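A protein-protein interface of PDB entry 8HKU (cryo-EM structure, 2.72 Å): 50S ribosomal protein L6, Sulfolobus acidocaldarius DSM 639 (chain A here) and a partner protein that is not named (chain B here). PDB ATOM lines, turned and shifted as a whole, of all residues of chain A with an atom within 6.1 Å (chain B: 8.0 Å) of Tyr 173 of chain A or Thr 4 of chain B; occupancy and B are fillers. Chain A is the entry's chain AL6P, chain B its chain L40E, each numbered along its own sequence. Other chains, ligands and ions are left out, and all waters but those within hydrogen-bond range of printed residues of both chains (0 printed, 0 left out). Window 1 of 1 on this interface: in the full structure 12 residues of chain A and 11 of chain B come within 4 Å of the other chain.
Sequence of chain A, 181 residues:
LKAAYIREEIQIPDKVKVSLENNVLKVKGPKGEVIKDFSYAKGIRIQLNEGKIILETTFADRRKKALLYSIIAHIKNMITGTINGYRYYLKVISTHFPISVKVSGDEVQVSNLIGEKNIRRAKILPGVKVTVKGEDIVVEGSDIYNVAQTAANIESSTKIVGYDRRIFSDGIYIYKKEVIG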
ATOM      1  N   TYR A  89     -10.167  30.437  36.967  1.00  0.00           N
ATOM      2  CA  TYR A  89      -8.952  29.710  36.644  1.00  0.00           C
ATOM      3  C   TYR A  89      -8.555  29.971  35.202  1.00  0.00           C
ATOM      4  O   TYR A  89      -9.410  30.069  34.318  1.00  0.00           O
ATOM      5  CB  TYR A  89      -9.124  28.209  36.861  1.00  0.00           C
ATOM      6  CG  TYR A  89      -9.360  27.809  38.293  1.00  0.00           C
ATOM      7  CD1 TYR A  89     -10.585  28.006  38.904  1.00  0.00           C
ATOM      8  CD2 TYR A  89      -8.349  27.225  39.033  1.00  0.00           C
ATOM      9  CE1 TYR A  89     -10.791  27.637  40.213  1.00  0.00           C
ATOM     10  CE2 TYR A  89      -8.546  26.854  40.335  1.00  0.00           C
ATOM     11  CZ  TYR A  89      -9.765  27.059  40.921  1.00  0.00           C
ATOM     12  OH  TYR A  89      -9.951  26.681  42.226  1.00  0.00           O
ATOM     13  N   LEU A  90      -7.254  30.096  34.974  1.00  0.00           N
ATOM     14  CA  LEU A  90      -6.690  30.222  33.642  1.00  0.00           C
ATOM     15  C   LEU A  90      -5.617  29.162  33.494  1.00  0.00           C
ATOM     16  O   LEU A  90      -4.867  28.903  34.433  1.00  0.00           O
ATOM     17  CB  LEU A  90      -6.100  31.607  33.410  1.00  0.00           C
ATOM     18  CG  LEU A  90      -7.059  32.789  33.503  1.00  0.00           C
ATOM     19  CD1 LEU A  90      -7.061  33.368  34.898  1.00  0.00           C
ATOM     20  CD2 LEU A  90      -6.681  33.846  32.496  1.00  0.00           C
ATOM     21  N   LYS A  91      -5.554  28.535  32.328  1.00  0.00           N
ATOM     22  CA  LYS A  91      -4.563  27.503  32.069  1.00  0.00           C
ATOM     23  C   LYS A  91      -3.481  28.045  31.147  1.00  0.00           C
ATOM     24  O   LYS A  91      -3.756  28.874  30.275  1.00  0.00           O
ATOM     25  CB  LYS A  91      -5.197  26.256  31.457  1.00  0.00           C
ATOM     26  CG  LYS A  91      -4.266  25.065  31.458  1.00  0.00           C
ATOM     27  CD  LYS A  91      -5.017  23.759  31.534  1.00  0.00           C
ATOM     28  CE  LYS A  91      -5.608  23.540  32.910  1.00  0.00           C
ATOM     29  NZ  LYS A  91      -4.559  23.328  33.936  1.00  0.00           N
ATOM     30  N   VAL A  92      -2.254  27.584  31.354  1.00  0.00           N
ATOM     31  CA  VAL A  92      -1.102  28.007  30.571  1.00  0.00           C
ATOM     32  C   VAL A  92      -0.747  26.870  29.625  1.00  0.00           C
ATOM     33  O   VAL A  92      -0.302  25.804  30.056  1.00  0.00           O
ATOM     34  CB  VAL A  92       0.081  28.380  31.471  1.00  0.00           C
ATOM     35  CG1 VAL A  92       1.281  28.745  30.637  1.00  0.00           C
ATOM     36  CG2 VAL A  92      -0.302  29.525  32.380  1.00  0.00           C
ATOM     37  N   ILE A  93      -0.933  27.098  28.331  1.00  0.00           N
ATOM     38  CA  ILE A  93      -0.734  26.081  27.309  1.00  0.00           C
ATOM     39  C   ILE A  93       0.450  26.501  26.452  1.00  0.00           C
ATOM     40  O   ILE A  93       0.470  27.612  25.909  1.00  0.00           O
ATOM     41  CB  ILE A  93      -1.994  25.891  26.454  1.00  0.00           C
ATOM     42  CG1 ILE A  93      -3.144  25.390  27.320  1.00  0.00           C
ATOM     43  CG2 ILE A  93      -1.731  24.912  25.335  1.00  0.00           C
ATOM     44  CD1 ILE A  93      -4.436  25.250  26.583  1.00  0.00           C
ATOM     45  N   GLU A 155      -5.954  37.156  29.457  1.00  0.00           N
ATOM     46  CA  GLU A 155      -6.379  36.427  28.268  1.00  0.00           C
ATOM     47  C   GLU A 155      -6.024  37.179  26.993  1.00  0.00           C
ATOM     48  O   GLU A 155      -5.548  36.584  26.022  1.00  0.00           O
ATOM     49  CB  GLU A 155      -7.886  36.200  28.345  1.00  0.00           C
ATOM     50  CG  GLU A 155      -8.488  35.418  27.207  1.00  0.00           C
ATOM     51  CD  GLU A 155      -7.998  34.007  27.172  1.00  0.00           C
ATOM     52  OE1 GLU A 155      -7.613  33.512  28.248  1.00  0.00           O
ATOM     53  OE2 GLU A 155      -8.017  33.388  26.089  1.00  0.00           O
ATOM     54  N   THR A 158      -1.975  37.733  25.711  1.00  0.00           N
ATOM     55  CA  THR A 158      -1.276  36.610  25.112  1.00  0.00           C
ATOM     56  C   THR A 158      -1.914  36.134  23.816  1.00  0.00           C
ATOM     57  O   THR A 158      -1.424  35.168  23.226  1.00  0.00           O
ATOM     58  CB  THR A 158      -1.210  35.450  26.102  1.00  0.00           C
ATOM     59  OG1 THR A 158      -2.502  34.851  26.215  1.00  0.00           O
ATOM     60  CG2 THR A 158      -0.793  35.953  27.461  1.00  0.00           C
ATOM     61  N   ILE A 167      -3.446  28.725  14.046  1.00  0.00           N
ATOM     62  CA  ILE A 167      -3.413  28.533  15.488  1.00  0.00           C
ATOM     63  C   ILE A 167      -3.045  27.094  15.818  1.00  0.00           C
ATOM     64  O   ILE A 167      -3.760  26.152  15.454  1.00  0.00           O
ATOM     65  CB  ILE A 167      -4.747  28.923  16.125  1.00  0.00           C
ATOM     66  CG1 ILE A 167      -5.068  30.386  15.831  1.00  0.00           C
ATOM     67  CG2 ILE A 167      -4.698  28.683  17.608  1.00  0.00           C
ATOM     68  CD1 ILE A 167      -4.230  31.361  16.596  1.00  0.00           C
ATOM     69  N   SER A 169      -2.563  26.420  19.198  1.00  0.00           N
ATOM     70  CA  SER A 169      -2.942  26.302  20.602  1.00  0.00           C
ATOM     71  C   SER A 169      -1.786  26.690  21.531  1.00  0.00           C
ATOM     72  O   SER A 169      -1.211  25.862  22.238  1.00  0.00           O
ATOM     73  CB  SER A 169      -3.431  24.877  20.896  1.00  0.00           C
ATOM     74  OG  SER A 169      -4.218  24.819  22.074  1.00  0.00           O
ATOM     75  N   ASP A 170      -1.444  27.975  21.498  1.00  0.00           N
ATOM     76  CA  ASP A 170      -0.378  28.509  22.340  1.00  0.00           C
ATOM     77  C   ASP A 170      -0.844  29.812  22.976  1.00  0.00           C
ATOM     78  O   ASP A 170      -1.074  30.800  22.275  1.00  0.00           O
ATOM     79  CB  ASP A 170       0.894  28.713  21.522  1.00  0.00           C
ATOM     80  CG  ASP A 170       2.140  28.494  22.332  1.00  0.00           C
ATOM     81  OD1 ASP A 170       2.185  28.961  23.484  1.00  0.00           O
ATOM     82  OD2 ASP A 170       3.076  27.857  21.815  1.00  0.00           O
ATOM     83  N   GLY A 171      -0.988  29.815  24.296  1.00  0.00           N
ATOM     84  CA  GLY A 171      -1.470  30.992  24.998  1.00  0.00           C
ATOM     85  C   GLY A 171      -1.940  30.627  26.396  1.00  0.00           C
ATOM     86  O   GLY A 171      -1.613  29.567  26.915  1.00  0.00           O
ATOM     87  N   ILE A 172      -2.704  31.542  26.987  1.00  0.00           N
ATOM     88  CA  ILE A 172      -3.307  31.364  28.304  1.00  0.00           C
ATOM     89  C   ILE A 172      -4.813  31.514  28.147  1.00  0.00           C
ATOM     90  O   ILE A 172      -5.278  32.512  27.589  1.00  0.00           O
ATOM     91  CB  ILE A 172      -2.760  32.382  29.319  1.00  0.00           C
ATOM     92  CG1 ILE A 172      -1.262  32.182  29.530  1.00  0.00           C
ATOM     93  CG2 ILE A 172      -3.491  32.271  30.634  1.00  0.00           C
ATOM     94  CD1 ILE A 172      -0.633  33.237  30.392  1.00  0.00           C
ATOM     95  N   TYR A 173      -5.575  30.538  28.649  1.00  0.00           N
ATOM     96  CA  TYR A 173      -7.003  30.446  28.371  1.00  0.00           C
ATOM     97  C   TYR A 173      -7.813  30.294  29.651  1.00  0.00           C
ATOM     98  O   TYR A 173      -7.362  29.679  30.618  1.00  0.00           O
ATOM     99  CB  TYR A 173      -7.296  29.274  27.441  1.00  0.00           C
ATOM    100  CG  TYR A 173      -6.525  29.325  26.148  1.00  0.00           C
ATOM    101  CD1 TYR A 173      -6.939  30.129  25.103  1.00  0.00           C
ATOM    102  CD2 TYR A 173      -5.377  28.575  25.974  1.00  0.00           C
ATOM    103  CE1 TYR A 173      -6.239  30.179  23.925  1.00  0.00           C
ATOM    104  CE2 TYR A 173      -4.671  28.620  24.797  1.00  0.00           C
ATOM    105  CZ  TYR A 173      -5.109  29.422  23.775  1.00  0.00           C
ATOM    106  OH  TYR A 173      -4.411  29.473  22.595  1.00  0.00           O
ATOM    107  N   ILE A 174      -9.031  30.847  29.635  1.00  0.00           N
ATOM    108  CA  ILE A 174      -9.918  30.773  30.792  1.00  0.00           C
ATOM    109  C   ILE A 174     -10.472  29.360  30.936  1.00  0.00           C
ATOM    110  O   ILE A 174     -10.722  28.656  29.952  1.00  0.00           O
ATOM    111  CB  ILE A 174     -11.058  31.801  30.685  1.00  0.00           C
ATOM    112  CG1 ILE A 174     -10.495  33.218  30.580  1.00  0.00           C
ATOM    113  CG2 ILE A 174     -11.950  31.709  31.902  1.00  0.00           C
ATOM    114  CD1 ILE A 174     -10.690  34.060  31.820  1.00  0.00           C
ATOM    115  N   TYR A 175     -10.675  28.943  32.183  1.00  0.00           N
ATOM    116  CA  TYR A 175     -10.870  27.543  32.530  1.00  0.00           C
ATOM    117  C   TYR A 175     -12.216  27.261  33.182  1.00  0.00           C
ATOM    118  O   TYR A 175     -12.962  26.411  32.687  1.00  0.00           O
ATOM    119  CB  TYR A 175      -9.696  27.127  33.433  1.00  0.00           C
ATOM    120  CG  TYR A 175      -9.532  25.664  33.694  1.00  0.00           C
ATOM    121  CD1 TYR A 175      -9.917  24.725  32.759  1.00  0.00           C
ATOM    122  CD2 TYR A 175      -8.929  25.225  34.858  1.00  0.00           C
ATOM    123  CE1 TYR A 175      -9.750  23.382  32.998  1.00  0.00           C
ATOM    124  CE2 TYR A 175      -8.753  23.891  35.104  1.00  0.00           C
ATOM    125  CZ  TYR A 175      -9.163  22.970  34.171  1.00  0.00           C
ATOM    126  OH  TYR A 175      -8.987  21.628  34.415  1.00  0.00           O
ATOM    127  N   MET B   1      -9.133  28.856  18.804  1.00  0.00           N
ATOM    128  CA  MET B   1      -9.393  30.217  19.239  1.00  0.00           C
ATOM    129  C   MET B   1      -8.435  30.656  20.338  1.00  0.00           C
ATOM    130  O   MET B   1      -8.217  29.927  21.304  1.00  0.00           O
ATOM    131  CB  MET B   1     -10.849  30.363  19.699  1.00  0.00           C
ATOM    132  CG  MET B   1     -11.253  29.575  20.933  1.00  0.00           C
ATOM    133  SD  MET B   1     -13.001  29.849  21.268  1.00  0.00           S
ATOM    134  CE  MET B   1     -13.296  28.840  22.718  1.00  0.00           C
ATOM    135  N   PRO B   2      -7.834  31.840  20.171  1.00  0.00           N
ATOM    136  CA  PRO B   2      -6.938  32.372  21.207  1.00  0.00           C
ATOM    137  C   PRO B   2      -7.651  33.092  22.344  1.00  0.00           C
ATOM    138  O   PRO B   2      -7.026  33.326  23.387  1.00  0.00           O
ATOM    139  CB  PRO B   2      -6.034  33.338  20.423  1.00  0.00           C
ATOM    140  CG  PRO B   2      -6.296  33.054  18.975  1.00  0.00           C
ATOM    141  CD  PRO B   2      -7.707  32.599  18.919  1.00  0.00           C
ATOM    142  N   LEU B   3      -8.926  33.447  22.185  1.00  0.00           N
ATOM    143  CA  LEU B   3      -9.708  34.099  23.238  1.00  0.00           C
ATOM    144  C   LEU B   3     -10.978  33.277  23.454  1.00  0.00           C
ATOM    145  O   LEU B   3     -11.962  33.445  22.726  1.00  0.00           O
ATOM    146  CB  LEU B   3     -10.038  35.544  22.869  1.00  0.00           C
ATOM    147  CG  LEU B   3      -8.856  36.477  22.579  1.00  0.00           C
ATOM    148  CD1 LEU B   3      -9.319  37.901  22.304  1.00  0.00           C
ATOM    149  CD2 LEU B   3      -7.864  36.455  23.719  1.00  0.00           C
ATOM    150  N   THR B   4     -10.961  32.396  24.455  1.00  0.00           N
ATOM    151  CA  THR B   4     -12.087  31.506  24.703  1.00  0.00           C
ATOM    152  C   THR B   4     -13.155  32.211  25.535  1.00  0.00           C
ATOM    153  O   THR B   4     -12.997  33.354  25.971  1.00  0.00           O
ATOM    154  CB  THR B   4     -11.637  30.225  25.400  1.00  0.00           C
ATOM    155  OG1 THR B   4     -11.383  30.493  26.782  1.00  0.00           O
ATOM    156  CG2 THR B   4     -10.401  29.660  24.747  1.00  0.00           C
ATOM    157  N   ASP B   5     -14.256  31.510  25.773  1.00  0.00           N
ATOM    158  CA  ASP B   5     -15.376  32.007  26.541  1.00  0.00           C
ATOM    159  C   ASP B   5     -15.303  31.451  27.956  1.00  0.00           C
ATOM    160  O   ASP B   5     -15.087  30.250  28.147  1.00  0.00           O
ATOM    161  CB  ASP B   5     -16.701  31.613  25.883  1.00  0.00           C
ATOM    162  CG  ASP B   5     -16.855  32.194  24.492  1.00  0.00           C
ATOM    163  OD1 ASP B   5     -16.669  33.418  24.334  1.00  0.00           O
ATOM    164  OD2 ASP B   5     -17.139  31.420  23.554  1.00  0.00           O
ATOM    165  N   PRO B   6     -15.480  32.303  28.964  1.00  0.00           N
ATOM    166  CA  PRO B   6     -14.987  31.980  30.311  1.00  0.00           C
ATOM    167  C   PRO B   6     -15.577  30.710  30.925  1.00  0.00           C
ATOM    168  O   PRO B   6     -14.829  29.771  31.210  1.00  0.00           O
ATOM    169  CB  PRO B   6     -15.342  33.240  31.114  1.00  0.00           C
ATOM    170  CG  PRO B   6     -16.373  33.961  30.291  1.00  0.00           C
ATOM    171  CD  PRO B   6     -16.031  33.662  28.882  1.00  0.00           C
ATOM    172  N   VAL B   7     -16.894  30.647  31.119  1.00  0.00           N
ATOM    173  CA  VAL B   7     -17.602  29.385  31.358  1.00  0.00           C
ATOM    174  C   VAL B   7     -18.757  29.341  30.371  1.00  0.00           C
ATOM    175  O   VAL B   7     -19.804  29.967  30.583  1.00  0.00           O
ATOM    176  CB  VAL B   7     -18.084  29.201  32.800  1.00  0.00           C
ATOM    177  CG1 VAL B   7     -19.142  28.118  32.857  1.00  0.00           C
ATOM    178  CG2 VAL B   7     -16.946  28.707  33.638  1.00  0.00           C
ATOM    179  N   LYS B   8     -18.553  28.611  29.286  1.00  0.00           N
ATOM    180  CA  LYS B   8     -19.451  28.503  28.156  1.00  0.00           C
ATOM    181  C   LYS B   8     -19.216  27.117  27.569  1.00  0.00           C
ATOM    182  O   LYS B   8     -18.715  26.222  28.258  1.00  0.00           O
ATOM    183  CB  LYS B   8     -19.193  29.651  27.168  1.00  0.00           C
ATOM    184  CG  LYS B   8     -20.000  30.913  27.437  1.00  0.00           C
ATOM    185  CD  LYS B   8     -19.254  31.973  28.254  1.00  0.00           C
ATOM    186  CE  LYS B   8     -19.927  33.339  28.109  1.00  0.00           C
ATOM    187  NZ  LYS B   8     -19.328  34.432  28.926  1.00  0.00           N
ATOM    188  N   LEU B   9     -19.574  26.927  26.300  1.00  0.00           N
ATOM    189  CA  LEU B   9     -19.163  25.735  25.564  1.00  0.00           C
ATOM    190  C   LEU B   9     -17.769  25.880  24.965  1.00  0.00           C
ATOM    191  O   LEU B   9     -17.480  25.284  23.918  1.00  0.00           O
ATOM    192  CB  LEU B   9     -20.184  25.393  24.479  1.00  0.00           C
ATOM    193  CG  LEU B   9     -21.395  24.589  24.957  1.00  0.00           C
ATOM    194  CD1 LEU B   9     -22.178  24.028  23.776  1.00  0.00           C
ATOM    195  CD2 LEU B   9     -20.965  23.471  25.900  1.00  0.00           C
ATOM    196  N   GLN B  10     -16.907  26.677  25.605  1.00  0.00           N
ATOM    197  CA  GLN B  10     -15.530  26.922  25.188  1.00  0.00           C
ATOM    198  C   GLN B  10     -14.773  25.629  24.928  1.00  0.00           C
ATOM    199  O   GLN B  10     -15.172  24.559  25.397  1.00  0.00           O
ATOM    200  CB  GLN B  10     -14.783  27.719  26.250  1.00  0.00           C
ATOM    201  CG  GLN B  10     -14.645  26.958  27.551  1.00  0.00           C
ATOM    202  CD  GLN B  10     -13.600  27.549  28.454  1.00  0.00           C
ATOM    203  OE1 GLN B  10     -12.834  28.420  28.044  1.00  0.00           O
ATOM    204  NE2 GLN B  10     -13.550  27.072  29.688  1.00  0.00           N
ATOM    205  N   ILE B  11     -13.671  25.718  24.187  1.00  0.00           N
ATOM    206  CA  ILE B  11     -13.130  24.523  23.560  1.00  0.00           C
ATOM    207  C   ILE B  11     -11.660  24.234  23.858  1.00  0.00           C
ATOM    208  O   ILE B  11     -11.330  23.139  24.322  1.00  0.00           O
ATOM    209  CB  ILE B  11     -13.370  24.602  22.047  1.00  0.00           C
ATOM    210  CG1 ILE B  11     -12.646  25.794  21.466  1.00  0.00           C
ATOM    211  CG2 ILE B  11     -14.831  24.744  21.787  1.00  0.00           C
ATOM    212  CD1 ILE B  11     -12.682  25.843  20.047  1.00  0.00           C
ATOM    213  N   VAL B  12     -10.767  25.198  23.597  1.00  0.00           N
ATOM    214  CA  VAL B  12      -9.345  24.891  23.476  1.00  0.00           C
ATOM    215  C   VAL B  12      -8.820  24.291  24.766  1.00  0.00           C
ATOM    216  O   VAL B  12      -7.773  23.634  24.774  1.00  0.00           O
ATOM    217  CB  VAL B  12      -8.568  26.150  23.046  1.00  0.00           C
ATOM    218  CG1 VAL B  12      -7.078  25.867  22.928  1.00  0.00           C
ATOM    219  CG2 VAL B  12      -9.116  26.652  21.731  1.00  0.00           C
ATOM    220  N   GLN B  13      -9.559  24.453  25.858  1.00  0.00           N
ATOM    221  CA  GLN B  13      -9.417  23.554  26.992  1.00  0.00           C
ATOM    222  C   GLN B  13     -10.042  22.208  26.610  1.00  0.00           C
ATOM    223  O   GLN B  13     -11.113  21.815  27.079  1.00  0.00           O
ATOM    224  CB  GLN B  13     -10.050  24.155  28.235  1.00  0.00           C
ATOM    225  CG  GLN B  13      -9.717  23.387  29.474  1.00  0.00           C
ATOM    226  CD  GLN B  13      -8.249  23.078  29.540  1.00  0.00           C
ATOM    227  OE1 GLN B  13      -7.427  23.979  29.659  1.00  0.00           O
ATOM    228  NE2 GLN B  13      -7.905  21.798  29.447  1.00  0.00           N
ATOM    229  N   ARG B  15     -11.104  20.993  23.472  1.00  0.00           N
ATOM    230  CA  ARG B  15     -12.117  20.866  22.423  1.00  0.00           C
ATOM    231  C   ARG B  15     -11.769  21.813  21.279  1.00  0.00           C
ATOM    232  O   ARG B  15     -10.892  22.672  21.397  1.00  0.00           O
ATOM    233  CB  ARG B  15     -13.528  21.178  22.935  1.00  0.00           C
ATOM    234  CG  ARG B  15     -14.233  20.088  23.693  1.00  0.00           C
ATOM    235  CD  ARG B  15     -15.593  20.578  24.128  1.00  0.00           C
ATOM    236  NE  ARG B  15     -15.437  21.685  25.060  1.00  0.00           N
ATOM    237  CZ  ARG B  15     -15.262  21.544  26.367  1.00  0.00           C
ATOM    238  NH1 ARG B  15     -15.216  20.350  26.932  1.00  0.00           N
ATOM    239  NH2 ARG B  15     -15.117  22.627  27.122  1.00  0.00           N
ATOM    240  N   LEU B  18     -15.553  25.390  17.603  1.00  0.00           N
ATOM    241  CA  LEU B  18     -15.200  26.803  17.522  1.00  0.00           C
ATOM    242  C   LEU B  18     -16.440  27.664  17.285  1.00  0.00           C
ATOM    243  O   LEU B  18     -17.576  27.272  17.562  1.00  0.00           O
ATOM    244  CB  LEU B  18     -14.148  27.011  16.435  1.00  0.00           C
ATOM    245  CG  LEU B  18     -12.688  26.772  16.821  1.00  0.00           C
ATOM    246  CD1 LEU B  18     -11.852  26.309  15.654  1.00  0.00           C
ATOM    247  CD2 LEU B  18     -12.108  28.042  17.397  1.00  0.00           C
ATOM    248  N   LYS B  19     -16.210  28.888  16.824  1.00  0.00           N
ATOM    249  CA  LYS B  19     -17.233  29.909  16.682  1.00  0.00           C
ATOM    250  C   LYS B  19     -17.887  29.845  15.300  1.00  0.00           C
ATOM    251  O   LYS B  19     -17.713  28.890  14.543  1.00  0.00           O
ATOM    252  CB  LYS B  19     -16.619  31.277  16.957  1.00  0.00           C
ATOM    253  CG  LYS B  19     -15.951  31.366  18.311  1.00  0.00           C
ATOM    254  CD  LYS B  19     -15.691  32.799  18.713  1.00  0.00           C
ATOM    255  CE  LYS B  19     -15.031  32.865  20.076  1.00  0.00           C
ATOM    256  NZ  LYS B  19     -15.751  32.019  21.065  1.00  0.00           N
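Of the 16 printed residues of chain B, 8 touch a printed residue of chain A.
Hydrophobic or aromatic side chains of chain B within 4 Å of the printed part of chain A: Pro 2, Leu 3, Pro 6 and Val 12.
Along chain B the printed residues that touch a printed residue of chain A span positions 1 to 13.
Among the printed residues, no Asp or Glu carboxylate lies within 4 Å of a Lys or Arg side-chain nitrogen of the other chain.
Among the printed residues, pairs that only touch across the chains: Lys 91 of chain A with Gln 13 of chain B (3.1 Å), Glu 155 of chain A with Leu 3 of chain B (3.3 Å), Glu 155 of chain A with Thr 4 of chain B (3.5 Å), Ile 167 of chain A with Pro 2 of chain B (3.6 Å), Ser 169 of chain A with Val 12 of chain B (3.2 Å), Tyr 173 of chain A with Met 1 of chain B (3.3 Å), Tyr 173 of chain A with Pro 2 of chain B (3.3 Å), Tyr 173 of chain A with Thr 4 of chain B (3.5 Å), Ile 174 of chain A with Thr 4 of chain B (3.7 Å), Ile 174 of chain A with Pro 6 of chain B (3.4 Å) and Tyr 175 of chain A with Gln 13 of chain B (3.5 Å).
OE2 of Glu 155 of chain A lies close to O of Pro 2 of chain B (2.9 Å).
O of Tyr 175 of chain A is in hydrogen-bond range of NE2 of Gln 10 of chain B (3.1 Å).
The side-chain amide oxygen of Gln 10 of chain B lies close to the backbone carbonyl oxygen of Ile 174 of chain A, at 2.9 Å.
The backbone NH (N) of Lys 91 of chain A is in hydrogen-bond range of the backbone carbonyl oxygen (O) of Tyr 173 of chain A, 2.7 Å away.
The backbone carbonyl oxygen (O) of Asp 5 of chain B lies close to the side-chain amide oxygen (OE1) of Gln 10 of chain B, at 2.9 Å.
The backbone carbonyl oxygen (O) of Pro 6 of chain B sits at hydrogen-bond distance from the side-chain amide nitrogen (NE2) of Gln 10 of chain B (3.4 Å).
The side-chain carboxylate (OE1) of Glu 155 of chain A lies within hydrogen-bond range of the backbone NH (N) of Ile 174 of chain A (3.3 Å).
The backbone carbonyl oxygen of Tyr 89 of chain A lies within hydrogen-bond range of the backbone NH of Tyr 175 of chain A (2.7 Å).
O of Ile 172 of chain A sits close to OE1 of Glu 155 of chain A, at 2.6 Å.
Thr 4 of chain B touches three residues of chain A.
Of the printed residues of chain B, Glu 155 of chain A touches Pro 2 (2.9 Å), Leu 3 (3.3 Å) and Thr 4 (3.5 Å).
Printed residues of chain A within 4 Å of Leu 3 of chain B: Glu 155.
Printed residues of chain B within 4 Å of Lys 91 of chain A: Gln 13 (3.1 Å).
Printed residues of chain A within 4 Å of Gln 13 of chain B: Lys 91 and Tyr 175.
Of the printed residues of chain B, Ile 174 of chain A touches Thr 4, Pro 6 and Gln 10.
Leu 90 of chain A touches none of the printed residues of chain B.
Ile 172 of chain A touches none of the printed residues of chain B.
The nearest residue of chain B that does not touch Tyr 173 of chain A is Val 12 of chain B (4.1 Å).
The nearest residue of chain A that does not touch Thr 4 of chain B is Tyr 175 of chain A (5.7 Å).
The nearest printed residue of chain A that does not touch Pro 2 of chain B is Ile 172 of chain A (4.6 Å).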
